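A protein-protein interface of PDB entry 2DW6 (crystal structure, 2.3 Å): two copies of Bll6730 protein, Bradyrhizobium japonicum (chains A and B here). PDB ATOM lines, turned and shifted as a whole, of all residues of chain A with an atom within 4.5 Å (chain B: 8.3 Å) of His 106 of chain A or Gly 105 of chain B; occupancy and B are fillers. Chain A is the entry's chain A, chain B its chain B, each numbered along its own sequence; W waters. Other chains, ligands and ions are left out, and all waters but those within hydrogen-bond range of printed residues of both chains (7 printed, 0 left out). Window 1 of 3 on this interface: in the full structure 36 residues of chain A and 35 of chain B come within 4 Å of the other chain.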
ATOM      1  N   ARG A  57       6.874  -2.356 -27.890  1.00  0.00           N
ATOM      2  CA  ARG A  57       7.783  -2.352 -26.751  1.00  0.00           C
ATOM      3  C   ARG A  57       8.342  -3.725 -26.371  1.00  0.00           C
ATOM      4  O   ARG A  57       9.108  -3.835 -25.416  1.00  0.00           O
ATOM      5  CB  ARG A  57       7.103  -1.713 -25.537  1.00  0.00           C
ATOM      6  CG  ARG A  57       6.404  -0.378 -25.824  1.00  0.00           C
ATOM      7  CD  ARG A  57       7.309   0.675 -26.472  1.00  0.00           C
ATOM      8  NE  ARG A  57       8.502   0.976 -25.682  1.00  0.00           N
ATOM      9  CZ  ARG A  57       9.169   2.124 -25.742  1.00  0.00           C
ATOM     10  NH1 ARG A  57       8.760   3.090 -26.555  1.00  0.00           N
ATOM     11  NH2 ARG A  57      10.250   2.309 -24.996  1.00  0.00           N
ATOM     12  N   GLY A 104      10.393   6.949 -11.042  1.00  0.00           N
ATOM     13  CA  GLY A 104      11.028   7.233 -12.317  1.00  0.00           C
ATOM     14  C   GLY A 104      11.292   5.950 -13.089  1.00  0.00           C
ATOM     15  O   GLY A 104      10.901   4.862 -12.655  1.00  0.00           O
ATOM     16  N   GLY A 105      11.957   6.071 -14.234  1.00  0.00           N
ATOM     17  CA  GLY A 105      12.266   4.902 -15.043  1.00  0.00           C
ATOM     18  C   GLY A 105      11.023   4.172 -15.517  1.00  0.00           C
ATOM     19  O   GLY A 105      10.897   2.957 -15.362  1.00  0.00           O
ATOM     20  N   HIS A 106      10.098   4.913 -16.111  1.00  0.00           N
ATOM     21  CA  HIS A 106       8.860   4.320 -16.587  1.00  0.00           C
ATOM     22  C   HIS A 106       8.958   3.781 -18.004  1.00  0.00           C
ATOM     23  O   HIS A 106       8.662   4.472 -18.976  1.00  0.00           O
ATOM     24  CB  HIS A 106       7.739   5.341 -16.463  1.00  0.00           C
ATOM     25  CG  HIS A 106       7.572   5.857 -15.071  1.00  0.00           C
ATOM     26  ND1 HIS A 106       7.400   5.021 -13.990  1.00  0.00           N
ATOM     27  CD2 HIS A 106       7.594   7.115 -14.576  1.00  0.00           C
ATOM     28  CE1 HIS A 106       7.324   5.744 -12.886  1.00  0.00           C
ATOM     29  NE2 HIS A 106       7.438   7.018 -13.214  1.00  0.00           N
ATOM     30  N   GLY A 107       9.399   2.532 -18.095  1.00  0.00           N
ATOM     31  CA  GLY A 107       9.550   1.856 -19.366  1.00  0.00           C
ATOM     32  C   GLY A 107       9.858   0.400 -19.065  1.00  0.00           C
ATOM     33  O   GLY A 107      10.493   0.097 -18.046  1.00  0.00           O
ATOM     34  N   ARG A 109       9.092  -2.085 -17.358  1.00  0.00           N
ATOM     35  CA  ARG A 109       8.332  -2.594 -16.227  1.00  0.00           C
ATOM     36  C   ARG A 109       6.893  -2.073 -16.319  1.00  0.00           C
ATOM     37  O   ARG A 109       5.961  -2.687 -15.804  1.00  0.00           O
ATOM     38  CB  ARG A 109       8.972  -2.173 -14.901  1.00  0.00           C
ATOM     39  CG  ARG A 109       8.880  -0.700 -14.593  1.00  0.00           C
ATOM     40  CD  ARG A 109       9.350  -0.409 -13.177  1.00  0.00           C
ATOM     41  NE  ARG A 109       9.206   1.005 -12.850  1.00  0.00           N
ATOM     42  CZ  ARG A 109       9.625   1.567 -11.721  1.00  0.00           C
ATOM     43  NH1 ARG A 109      10.226   0.837 -10.788  1.00  0.00           N
ATOM     44  NH2 ARG A 109       9.455   2.868 -11.528  1.00  0.00           N
ATOM     45  N   SER A 110       6.722  -0.938 -16.988  1.00  0.00           N
ATOM     46  CA  SER A 110       5.396  -0.358 -17.162  1.00  0.00           C
ATOM     47  C   SER A 110       4.569  -1.261 -18.084  1.00  0.00           C
ATOM     48  O   SER A 110       3.343  -1.335 -17.977  1.00  0.00           O
ATOM     49  CB  SER A 110       5.515   1.040 -17.768  1.00  0.00           C
ATOM     50  OG  SER A 110       6.215   0.991 -19.002  1.00  0.00           O
ATOM     51  N   ASN A 266       4.170   6.779 -26.410  1.00  0.00           N
ATOM     52  CA  ASN A 266       5.433   6.442 -25.767  1.00  0.00           C
ATOM     53  C   ASN A 266       5.695   7.105 -24.410  1.00  0.00           C
ATOM     54  O   ASN A 266       6.848   7.244 -23.988  1.00  0.00           O
ATOM     55  CB  ASN A 266       6.598   6.707 -26.726  1.00  0.00           C
ATOM     56  CG  ASN A 266       6.599   5.751 -27.910  1.00  0.00           C
ATOM     57  OD1 ASN A 266       6.509   4.532 -27.736  1.00  0.00           O
ATOM     58  ND2 ASN A 266       6.702   6.295 -29.116  1.00  0.00           N
ATOM     59  N   PHE A 268       4.702   6.491 -20.569  1.00  0.00           N
ATOM     60  CA  PHE A 268       4.136   5.383 -19.807  1.00  0.00           C
ATOM     61  C   PHE A 268       3.776   5.551 -18.339  1.00  0.00           C
ATOM     62  O   PHE A 268       3.736   4.565 -17.603  1.00  0.00           O
ATOM     63  CB  PHE A 268       5.071   4.182 -19.965  1.00  0.00           C
ATOM     64  CG  PHE A 268       5.438   3.897 -21.393  1.00  0.00           C
ATOM     65  CD1 PHE A 268       4.467   3.482 -22.306  1.00  0.00           C
ATOM     66  CD2 PHE A 268       6.747   4.074 -21.839  1.00  0.00           C
ATOM     67  CE1 PHE A 268       4.793   3.249 -23.648  1.00  0.00           C
ATOM     68  CE2 PHE A 268       7.090   3.842 -23.183  1.00  0.00           C
ATOM     69  CZ  PHE A 268       6.111   3.428 -24.090  1.00  0.00           C
ATOM     70  N   SER A 269       3.495   6.778 -17.914  1.00  0.00           N
ATOM     71  CA  SER A 269       3.123   7.025 -16.527  1.00  0.00           C
ATOM     72  C   SER A 269       2.280   8.292 -16.462  1.00  0.00           C
ATOM     73  O   SER A 269       2.291   9.095 -17.396  1.00  0.00           O
ATOM     74  CB  SER A 269       4.374   7.198 -15.665  1.00  0.00           C
ATOM     75  OG  SER A 269       5.044   8.399 -15.989  1.00  0.00           O
ATOM     76  N   GLN A 271       2.856  10.630 -14.462  1.00  0.00           N
ATOM     77  CA  GLN A 271       3.844  11.696 -14.274  1.00  0.00           C
ATOM     78  C   GLN A 271       4.303  12.218 -15.632  1.00  0.00           C
ATOM     79  O   GLN A 271       4.400  13.430 -15.838  1.00  0.00           O
ATOM     80  CB  GLN A 271       5.078  11.212 -13.498  1.00  0.00           C
ATOM     81  CG  GLN A 271       4.824  10.910 -12.032  1.00  0.00           C
ATOM     82  CD  GLN A 271       4.484   9.460 -11.795  1.00  0.00           C
ATOM     83  OE1 GLN A 271       3.823   8.819 -12.620  1.00  0.00           O
ATOM     84  NE2 GLN A 271       4.922   8.932 -10.660  1.00  0.00           N
ATOM     85  N   ASP A 272       4.591  11.302 -16.556  1.00  0.00           N
ATOM     86  CA  ASP A 272       5.032  11.699 -17.890  1.00  0.00           C
ATOM     87  C   ASP A 272       3.888  12.395 -18.645  1.00  0.00           C
ATOM     88  O   ASP A 272       4.113  13.359 -19.380  1.00  0.00           O
ATOM     89  CB  ASP A 272       5.541  10.482 -18.682  1.00  0.00           C
ATOM     90  CG  ASP A 272       6.907   9.989 -18.200  1.00  0.00           C
ATOM     91  OD1 ASP A 272       7.001   8.829 -17.728  1.00  0.00           O
ATOM     92  OD2 ASP A 272       7.887  10.767 -18.294  1.00  0.00           O
ATOM     93  N   TYR A 297       1.506   0.641 -17.020  1.00  0.00           N
ATOM     94  CA  TYR A 297       1.087   0.202 -15.684  1.00  0.00           C
ATOM     95  C   TYR A 297      -0.409  -0.100 -15.577  1.00  0.00           C
ATOM     96  O   TYR A 297      -0.950  -0.181 -14.480  1.00  0.00           O
ATOM     97  CB  TYR A 297       1.480   1.244 -14.635  1.00  0.00           C
ATOM     98  CG  TYR A 297       2.967   1.497 -14.535  1.00  0.00           C
ATOM     99  CD1 TYR A 297       3.806   0.607 -13.859  1.00  0.00           C
ATOM    100  CD2 TYR A 297       3.535   2.646 -15.092  1.00  0.00           C
ATOM    101  CE1 TYR A 297       5.178   0.861 -13.734  1.00  0.00           C
ATOM    102  CE2 TYR A 297       4.896   2.909 -14.976  1.00  0.00           C
ATOM    103  CZ  TYR A 297       5.711   2.017 -14.294  1.00  0.00           C
ATOM    104  OH  TYR A 297       7.050   2.303 -14.167  1.00  0.00           O
ATOM    105  N   TYR B  23      11.148   5.474   0.195  1.00  0.00           N
ATOM    106  CA  TYR B  23      10.374   4.892  -0.895  1.00  0.00           C
ATOM    107  C   TYR B  23      10.419   3.375  -1.033  1.00  0.00           C
ATOM    108  O   TYR B  23       9.409   2.745  -1.361  1.00  0.00           O
ATOM    109  CB  TYR B  23      10.853   5.504  -2.214  1.00  0.00           C
ATOM    110  CG  TYR B  23       9.770   5.780  -3.234  1.00  0.00           C
ATOM    111  CD1 TYR B  23       9.393   7.092  -3.534  1.00  0.00           C
ATOM    112  CD2 TYR B  23       9.140   4.741  -3.916  1.00  0.00           C
ATOM    113  CE1 TYR B  23       8.421   7.362  -4.488  1.00  0.00           C
ATOM    114  CE2 TYR B  23       8.163   5.003  -4.877  1.00  0.00           C
ATOM    115  CZ  TYR B  23       7.812   6.316  -5.156  1.00  0.00           C
ATOM    116  OH  TYR B  23       6.854   6.589  -6.101  1.00  0.00           O
ATOM    117  N   ARG B  57      17.687  -0.385  -9.078  1.00  0.00           N
ATOM    118  CA  ARG B  57      16.825  -0.695 -10.208  1.00  0.00           C
ATOM    119  C   ARG B  57      16.746  -2.170 -10.574  1.00  0.00           C
ATOM    120  O   ARG B  57      16.066  -2.523 -11.542  1.00  0.00           O
ATOM    121  CB  ARG B  57      17.251   0.116 -11.434  1.00  0.00           C
ATOM    122  CG  ARG B  57      17.492   1.590 -11.155  1.00  0.00           C
ATOM    123  CD  ARG B  57      16.293   2.291 -10.513  1.00  0.00           C
ATOM    124  NE  ARG B  57      15.074   2.187 -11.314  1.00  0.00           N
ATOM    125  CZ  ARG B  57      14.071   3.068 -11.268  1.00  0.00           C
ATOM    126  NH1 ARG B  57      14.141   4.127 -10.464  1.00  0.00           N
ATOM    127  NH2 ARG B  57      12.991   2.891 -12.018  1.00  0.00           N
ATOM    128  N   ARG B  67      17.484  -9.258 -25.648  1.00  0.00           N
ATOM    129  CA  ARG B  67      17.456  -8.185 -26.616  1.00  0.00           C
ATOM    130  C   ARG B  67      18.760  -7.512 -27.013  1.00  0.00           C
ATOM    131  O   ARG B  67      19.021  -7.323 -28.197  1.00  0.00           O
ATOM    132  CB  ARG B  67      16.462  -7.119 -26.144  1.00  0.00           C
ATOM    133  CG  ARG B  67      15.413  -6.780 -27.183  1.00  0.00           C
ATOM    134  CD  ARG B  67      14.718  -5.467 -26.871  1.00  0.00           C
ATOM    135  NE  ARG B  67      13.706  -5.657 -25.858  1.00  0.00           N
ATOM    136  CZ  ARG B  67      13.184  -4.686 -25.127  1.00  0.00           C
ATOM    137  NH1 ARG B  67      13.573  -3.430 -25.287  1.00  0.00           N
ATOM    138  NH2 ARG B  67      12.273  -4.988 -24.219  1.00  0.00           N
ATOM    139  N   MET B  98      21.155  -0.736 -29.848  1.00  0.00           N
ATOM    140  CA  MET B  98      19.961   0.089 -29.730  1.00  0.00           C
ATOM    141  C   MET B  98      19.032   0.050 -30.945  1.00  0.00           C
ATOM    142  O   MET B  98      18.041   0.781 -30.984  1.00  0.00           O
ATOM    143  CB  MET B  98      20.333   1.541 -29.426  1.00  0.00           C
ATOM    144  CG  MET B  98      20.668   1.807 -27.963  1.00  0.00           C
ATOM    145  SD  MET B  98      19.349   1.292 -26.817  1.00  0.00           S
ATOM    146  CE  MET B  98      18.140   2.592 -27.080  1.00  0.00           C
ATOM    147  N   GLU B 101      14.636  -0.087 -31.181  1.00  0.00           N
ATOM    148  CA  GLU B 101      14.180   0.322 -29.863  1.00  0.00           C
ATOM    149  C   GLU B 101      13.405   1.624 -30.072  1.00  0.00           C
ATOM    150  O   GLU B 101      13.960   2.597 -30.571  1.00  0.00           O
ATOM    151  CB  GLU B 101      15.370   0.575 -28.944  1.00  0.00           C
ATOM    152  CG  GLU B 101      16.107  -0.683 -28.501  1.00  0.00           C
ATOM    153  CD  GLU B 101      15.227  -1.628 -27.695  1.00  0.00           C
ATOM    154  OE1 GLU B 101      14.504  -1.163 -26.789  1.00  0.00           O
ATOM    155  OE2 GLU B 101      15.266  -2.844 -27.961  1.00  0.00           O
ATOM    156  N   LYS B 102      12.121   1.637 -29.717  1.00  0.00           N
ATOM    157  CA  LYS B 102      11.307   2.837 -29.892  1.00  0.00           C
ATOM    158  C   LYS B 102      11.658   3.893 -28.850  1.00  0.00           C
ATOM    159  O   LYS B 102      12.118   3.565 -27.757  1.00  0.00           O
ATOM    160  CB  LYS B 102       9.812   2.494 -29.817  1.00  0.00           C
ATOM    161  CG  LYS B 102       9.289   1.775 -31.060  1.00  0.00           C
ATOM    162  CD  LYS B 102       7.785   1.477 -30.990  1.00  0.00           C
ATOM    163  CE  LYS B 102       6.950   2.755 -30.918  1.00  0.00           C
ATOM    164  NZ  LYS B 102       5.483   2.476 -30.966  1.00  0.00           N
ATOM    165  N   PRO B 103      11.453   5.182 -29.185  1.00  0.00           N
ATOM    166  CA  PRO B 103      11.744   6.309 -28.292  1.00  0.00           C
ATOM    167  C   PRO B 103      10.902   6.328 -27.018  1.00  0.00           C
ATOM    168  O   PRO B 103       9.844   5.703 -26.949  1.00  0.00           O
ATOM    169  CB  PRO B 103      11.494   7.526 -29.183  1.00  0.00           C
ATOM    170  CG  PRO B 103      10.407   7.039 -30.113  1.00  0.00           C
ATOM    171  CD  PRO B 103      10.895   5.658 -30.467  1.00  0.00           C
ATOM    172  N   GLY B 104      11.381   7.053 -26.013  1.00  0.00           N
ATOM    173  CA  GLY B 104      10.677   7.125 -24.747  1.00  0.00           C
ATOM    174  C   GLY B 104      10.841   5.836 -23.960  1.00  0.00           C
ATOM    175  O   GLY B 104      11.559   4.922 -24.384  1.00  0.00           O
ATOM    176  N   GLY B 105      10.178   5.757 -22.809  1.00  0.00           N
ATOM    177  CA  GLY B 105      10.263   4.563 -21.986  1.00  0.00           C
ATOM    178  C   GLY B 105      11.676   4.278 -21.510  1.00  0.00           C
ATOM    179  O   GLY B 105      12.181   3.167 -21.659  1.00  0.00           O
ATOM    180  N   HIS B 106      12.312   5.282 -20.924  1.00  0.00           N
ATOM    181  CA  HIS B 106      13.674   5.132 -20.444  1.00  0.00           C
ATOM    182  C   HIS B 106      13.743   4.614 -19.012  1.00  0.00           C
ATOM    183  O   HIS B 106      13.807   5.379 -18.043  1.00  0.00           O
ATOM    184  CB  HIS B 106      14.412   6.460 -20.589  1.00  0.00           C
ATOM    185  CG  HIS B 106      14.398   6.987 -21.990  1.00  0.00           C
ATOM    186  ND1 HIS B 106      14.827   6.241 -23.064  1.00  0.00           N
ATOM    187  CD2 HIS B 106      13.990   8.174 -22.498  1.00  0.00           C
ATOM    188  CE1 HIS B 106      14.687   6.945 -24.174  1.00  0.00           C
ATOM    189  NE2 HIS B 106      14.182   8.122 -23.857  1.00  0.00           N
ATOM    190  N   GLY B 107      13.724   3.292 -18.904  1.00  0.00           N
ATOM    191  CA  GLY B 107      13.791   2.615 -17.625  1.00  0.00           C
ATOM    192  C   GLY B 107      13.982   1.137 -17.915  1.00  0.00           C
ATOM    193  O   GLY B 107      13.495   0.644 -18.939  1.00  0.00           O
ATOM    194  N   GLU B 108      14.706   0.434 -17.043  1.00  0.00           N
ATOM    195  CA  GLU B 108      14.941  -1.004 -17.215  1.00  0.00           C
ATOM    196  C   GLU B 108      15.918  -1.294 -18.368  1.00  0.00           C
ATOM    197  O   GLU B 108      17.032  -1.779 -18.137  1.00  0.00           O
ATOM    198  CB  GLU B 108      13.606  -1.712 -17.456  1.00  0.00           C
ATOM    199  CG  GLU B 108      13.175  -2.729 -16.397  1.00  0.00           C
ATOM    200  CD  GLU B 108      13.131  -2.186 -14.969  1.00  0.00           C
ATOM    201  OE1 GLU B 108      12.439  -1.182 -14.691  1.00  0.00           O
ATOM    202  OE2 GLU B 108      13.792  -2.790 -14.108  1.00  0.00           O
ATOM    203  N   ARG B 109      15.517  -0.999 -19.604  1.00  0.00           N
ATOM    204  CA  ARG B 109      16.414  -1.235 -20.731  1.00  0.00           C
ATOM    205  C   ARG B 109      17.609  -0.283 -20.639  1.00  0.00           C
ATOM    206  O   ARG B 109      18.700  -0.590 -21.135  1.00  0.00           O
ATOM    207  CB  ARG B 109      15.692  -1.052 -22.071  1.00  0.00           C
ATOM    208  CG  ARG B 109      15.304   0.363 -22.388  1.00  0.00           C
ATOM    209  CD  ARG B 109      14.771   0.465 -23.800  1.00  0.00           C
ATOM    210  NE  ARG B 109      14.446   1.844 -24.137  1.00  0.00           N
ATOM    211  CZ  ARG B 109      13.860   2.222 -25.268  1.00  0.00           C
ATOM    212  NH1 ARG B 109      13.526   1.315 -26.183  1.00  0.00           N
ATOM    213  NH2 ARG B 109      13.612   3.510 -25.482  1.00  0.00           N
ATOM    214  N   SER B 110      17.400   0.865 -19.999  1.00  0.00           N
ATOM    215  CA  SER B 110      18.466   1.841 -19.823  1.00  0.00           C
ATOM    216  C   SER B 110      19.537   1.259 -18.887  1.00  0.00           C
ATOM    217  O   SER B 110      20.723   1.596 -18.985  1.00  0.00           O
ATOM    218  CB  SER B 110      17.903   3.126 -19.226  1.00  0.00           C
ATOM    219  OG  SER B 110      17.235   2.849 -18.003  1.00  0.00           O
ATOM    220  N   ASP B 243       8.920  13.447  -6.477  1.00  0.00           N
ATOM    221  CA  ASP B 243       9.002  12.544  -7.616  1.00  0.00           C
ATOM    222  C   ASP B 243      10.019  13.087  -8.614  1.00  0.00           C
ATOM    223  O   ASP B 243       9.986  14.265  -8.962  1.00  0.00           O
ATOM    224  CB  ASP B 243       7.618  12.395  -8.261  1.00  0.00           C
ATOM    225  CG  ASP B 243       7.594  11.346  -9.357  1.00  0.00           C
ATOM    226  OD1 ASP B 243       8.105  11.621 -10.466  1.00  0.00           O
ATOM    227  OD2 ASP B 243       7.069  10.240  -9.106  1.00  0.00           O
ATOM    228  N   PRO B 244      10.944  12.233  -9.085  1.00  0.00           N
ATOM    229  CA  PRO B 244      11.979  12.654 -10.040  1.00  0.00           C
ATOM    230  C   PRO B 244      11.476  13.328 -11.320  1.00  0.00           C
ATOM    231  O   PRO B 244      12.226  14.058 -11.982  1.00  0.00           O
ATOM    232  CB  PRO B 244      12.747  11.356 -10.312  1.00  0.00           C
ATOM    233  CG  PRO B 244      11.714  10.297 -10.090  1.00  0.00           C
ATOM    234  CD  PRO B 244      10.999  10.779  -8.860  1.00  0.00           C
ATOM    235  N   LEU B 245      10.210  13.102 -11.656  1.00  0.00           N
ATOM    236  CA  LEU B 245       9.628  13.694 -12.859  1.00  0.00           C
ATOM    237  C   LEU B 245       8.732  14.916 -12.615  1.00  0.00           C
ATOM    238  O   LEU B 245       8.268  15.551 -13.570  1.00  0.00           O
ATOM    239  CB  LEU B 245       8.853  12.627 -13.634  1.00  0.00           C
ATOM    240  CG  LEU B 245       9.721  11.540 -14.272  1.00  0.00           C
ATOM    241  CD1 LEU B 245       8.832  10.430 -14.789  1.00  0.00           C
ATOM    242  CD2 LEU B 245      10.560  12.137 -15.396  1.00  0.00           C
ATOM    243  N   ASN B 266      17.289   9.115 -10.663  1.00  0.00           N
ATOM    244  CA  ASN B 266      16.210   8.375 -11.301  1.00  0.00           C
ATOM    245  C   ASN B 266      15.748   8.898 -12.664  1.00  0.00           C
ATOM    246  O   ASN B 266      14.609   8.665 -13.081  1.00  0.00           O
ATOM    247  CB  ASN B 266      15.021   8.262 -10.348  1.00  0.00           C
ATOM    248  CG  ASN B 266      15.323   7.363  -9.156  1.00  0.00           C
ATOM    249  OD1 ASN B 266      15.794   6.227  -9.320  1.00  0.00           O
ATOM    250  ND2 ASN B 266      15.055   7.862  -7.952  1.00  0.00           N
ATOM    251  N   LEU B 267      16.629   9.622 -13.346  1.00  0.00           N
ATOM    252  CA  LEU B 267      16.349  10.121 -14.693  1.00  0.00           C
ATOM    253  C   LEU B 267      17.379   9.342 -15.511  1.00  0.00           C
ATOM    254  O   LEU B 267      18.580   9.428 -15.259  1.00  0.00           O
ATOM    255  CB  LEU B 267      16.566  11.641 -14.783  1.00  0.00           C
ATOM    256  CG  LEU B 267      15.574  12.483 -13.963  1.00  0.00           C
ATOM    257  CD1 LEU B 267      15.786  13.956 -14.266  1.00  0.00           C
ATOM    258  CD2 LEU B 267      14.149  12.088 -14.289  1.00  0.00           C
ATOM    259  N   PHE B 268      16.907   8.582 -16.490  1.00  0.00           N
ATOM    260  CA  PHE B 268      17.798   7.714 -17.241  1.00  0.00           C
ATOM    261  C   PHE B 268      18.080   7.978 -18.712  1.00  0.00           C
ATOM    262  O   PHE B 268      18.428   7.049 -19.441  1.00  0.00           O
ATOM    263  CB  PHE B 268      17.294   6.286 -17.068  1.00  0.00           C
ATOM    264  CG  PHE B 268      17.030   5.920 -15.637  1.00  0.00           C
ATOM    265  CD1 PHE B 268      18.079   5.855 -14.719  1.00  0.00           C
ATOM    266  CD2 PHE B 268      15.737   5.656 -15.197  1.00  0.00           C
ATOM    267  CE1 PHE B 268      17.845   5.528 -13.378  1.00  0.00           C
ATOM    268  CE2 PHE B 268      15.490   5.329 -13.858  1.00  0.00           C
ATOM    269  CZ  PHE B 268      16.550   5.263 -12.945  1.00  0.00           C
ATOM    270  N   SER B 269      17.949   9.223 -19.154  1.00  0.00           N
ATOM    271  CA  SER B 269      18.227   9.557 -20.552  1.00  0.00           C
ATOM    272  C   SER B 269      18.612  11.025 -20.635  1.00  0.00           C
ATOM    273  O   SER B 269      18.332  11.798 -19.711  1.00  0.00           O
ATOM    274  CB  SER B 269      16.989   9.308 -21.424  1.00  0.00           C
ATOM    275  OG  SER B 269      15.958  10.246 -21.125  1.00  0.00           O
ATOM    276  N   ASP B 272      15.444  13.131 -20.565  1.00  0.00           N
ATOM    277  CA  ASP B 272      14.897  13.383 -19.238  1.00  0.00           C
ATOM    278  C   ASP B 272      15.753  14.414 -18.499  1.00  0.00           C
ATOM    279  O   ASP B 272      15.234  15.261 -17.781  1.00  0.00           O
ATOM    280  CB  ASP B 272      14.808  12.080 -18.425  1.00  0.00           C
ATOM    281  CG  ASP B 272      13.675  11.157 -18.899  1.00  0.00           C
ATOM    282  OD1 ASP B 272      13.969  10.027 -19.364  1.00  0.00           O
ATOM    283  OD2 ASP B 272      12.490  11.561 -18.803  1.00  0.00           O
ATOM    284  N   TYR B 297      21.819   4.046 -19.982  1.00  0.00           N
ATOM    285  CA  TYR B 297      22.367   3.753 -21.307  1.00  0.00           C
ATOM    286  C   TYR B 297      23.886   3.948 -21.403  1.00  0.00           C
ATOM    287  O   TYR B 297      24.442   4.030 -22.500  1.00  0.00           O
ATOM    288  CB  TYR B 297      21.659   4.604 -22.362  1.00  0.00           C
ATOM    289  CG  TYR B 297      20.170   4.355 -22.460  1.00  0.00           C
ATOM    290  CD1 TYR B 297      19.671   3.237 -23.122  1.00  0.00           C
ATOM    291  CD2 TYR B 297      19.257   5.260 -21.922  1.00  0.00           C
ATOM    292  CE1 TYR B 297      18.297   3.029 -23.254  1.00  0.00           C
ATOM    293  CE2 TYR B 297      17.885   5.062 -22.045  1.00  0.00           C
ATOM    294  CZ  TYR B 297      17.411   3.947 -22.711  1.00  0.00           C
ATOM    295  OH  TYR B 297      16.055   3.746 -22.834  1.00  0.00           O
HETATM  296  O   HOH W   1      11.154   1.130 -22.782  1.00  0.00           O
HETATM  297  O   HOH W   2       5.151  15.029 -13.538  1.00  0.00           O
HETATM  298  O   HOH W   3      10.788   9.756 -18.329  1.00  0.00           O
HETATM  299  O   HOH W   4       7.751   8.405 -10.973  1.00  0.00           O
HETATM  300  O   HOH W   5      12.710   1.282 -14.086  1.00  0.00           O
HETATM  301  O   HOH W   6       8.446   7.866 -21.935  1.00  0.00           O
HETATM  302  O   HOH W   7      12.606   8.459 -15.239  1.00  0.00           O
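The guanidinium group (NH1) of Arg 57 of chain A lies within hydrogen-bond range of the backbone carbonyl oxygen (O) of Pro 103 of chain B, 2.9 Å away.
The backbone carbonyl oxygen (O) of Gly 104 of chain B lies within hydrogen-bond range of the guanidinium group (NH2) of Arg 57 of chain A.
The guanidinium group (NH2) of Arg 57 of chain B is in hydrogen-bond range of the backbone carbonyl oxygen (O) of Gly 104 of chain A (2.9 Å).
The side-chain amide nitrogen of Gln 271 of chain A sits at hydrogen-bond distance from the side-chain carboxylate of Asp 243 of chain B, at 3.0 Å.
The backbone carbonyl oxygen (O) of Gly 107 of chain A lies close to the backbone carbonyl oxygen (O) of Gly 107 of chain B (3.2 Å).
The side-chain hydroxyl (OH) of Tyr 297 of chain A lies within hydrogen-bond range of the guanidinium group (NE) of Arg 109 of chain A.
The side-chain hydroxyl (OH) of Tyr 297 of chain B is in hydrogen-bond range of the guanidinium group (NE) of Arg 109 of chain B (2.8 Å).
Among the printed residues, pairs that only touch across the chains: Arg 57 of chain A with Arg 67 of chain B, Arg 57 of chain A with Lys 102 of chain B, Arg 57 of chain A with Gly 105 of chain B, Arg 57 of chain A with Arg 109 of chain B, Gly 104 of chain A with Pro 244 of chain B, Gly 104 of chain A with Asn 266 of chain B, Gly 105 of chain A with Arg 57 of chain B, Gly 105 of chain A with His 106 of chain B, Gly 105 of chain A with Gly 107 of chain B, Gly 105 of chain A with Asn 266 of chain B, Gly 105 of chain A with Phe 268 of chain B, His 106 of chain A with Gly 105 of chain B, His 106 of chain A with Leu 245 of chain B, Gly 107 of chain A with Gly 105 of chain B, Gly 107 of chain A with Glu 108 of chain B, Arg 109 of chain A with Arg 57 of chain B, Arg 109 of chain A with Glu 108 of chain B, Asn 266 of chain A with Lys 102 of chain B, Asn 266 of chain A with Pro 103 of chain B, Asn 266 of chain A with Gly 104 of chain B, Asn 266 of chain A with Gly 105 of chain B, Phe 268 of chain A with Gly 105 of chain B and Asp 272 of chain A with Leu 245 of chain B.
Of chain A, only Arg 57 (3.8 Å), His 106 (3.4 Å), Gly 107 (3.7 Å), Asn 266 (3.8 Å) and Phe 268 (3.5 Å) come within 4 Å of Gly 105 of chain B.
Gly 105 of chain A touches five residues of chain B.
Gly 107 of chain A touches just these residues of chain B: Gly 105, Gly 107 and Glu 108.
Of the printed residues of chain A, Leu 245 of chain B touches His 106 (3.5 Å) and Asp 272 (3.6 Å).
Of the printed residues of chain A, Arg 67 of chain B touches Arg 57.
Tyr 297 of chain B touches none of the printed residues of chain A.
Of the 23 printed residues of chain B, 15 touch a printed residue of chain A.
Hydrophobic or aromatic side chains of chain B that line the printed part of chain A: Pro 103, Pro 244, Leu 245 and Phe 268.
Printed residues of chain A that touch a printed residue of chain B: Arg 57, Gly 104, Gly 105, His 106, Gly 107, Arg 109, Asn 266, Phe 268, Gln 271 and Asp 272.
Hydrophobic or aromatic side chains of chain A that line the printed part of chain B: His 106 and Phe 268.
Along chain A the printed residues that touch a printed residue of chain B span positions 57 to 272.
Arg 57 of chain A touches Gly 104 of chain B, and with the chains exchanged Gly 104 of chain A touches Arg 57 of chain B.
Gly 107 of chain A touches its own counterpart, Gly 107 of chain B.
Water W1 lies within hydrogen-bond range of O of Gly 105 of chain B (2.5 Å) and NH2 of Arg 57 of chain A (2.7 Å).
Water W2 bridges O of Gln 271 of chain A (2.9 Å) and O of Leu 245 of chain B (3.2 Å).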
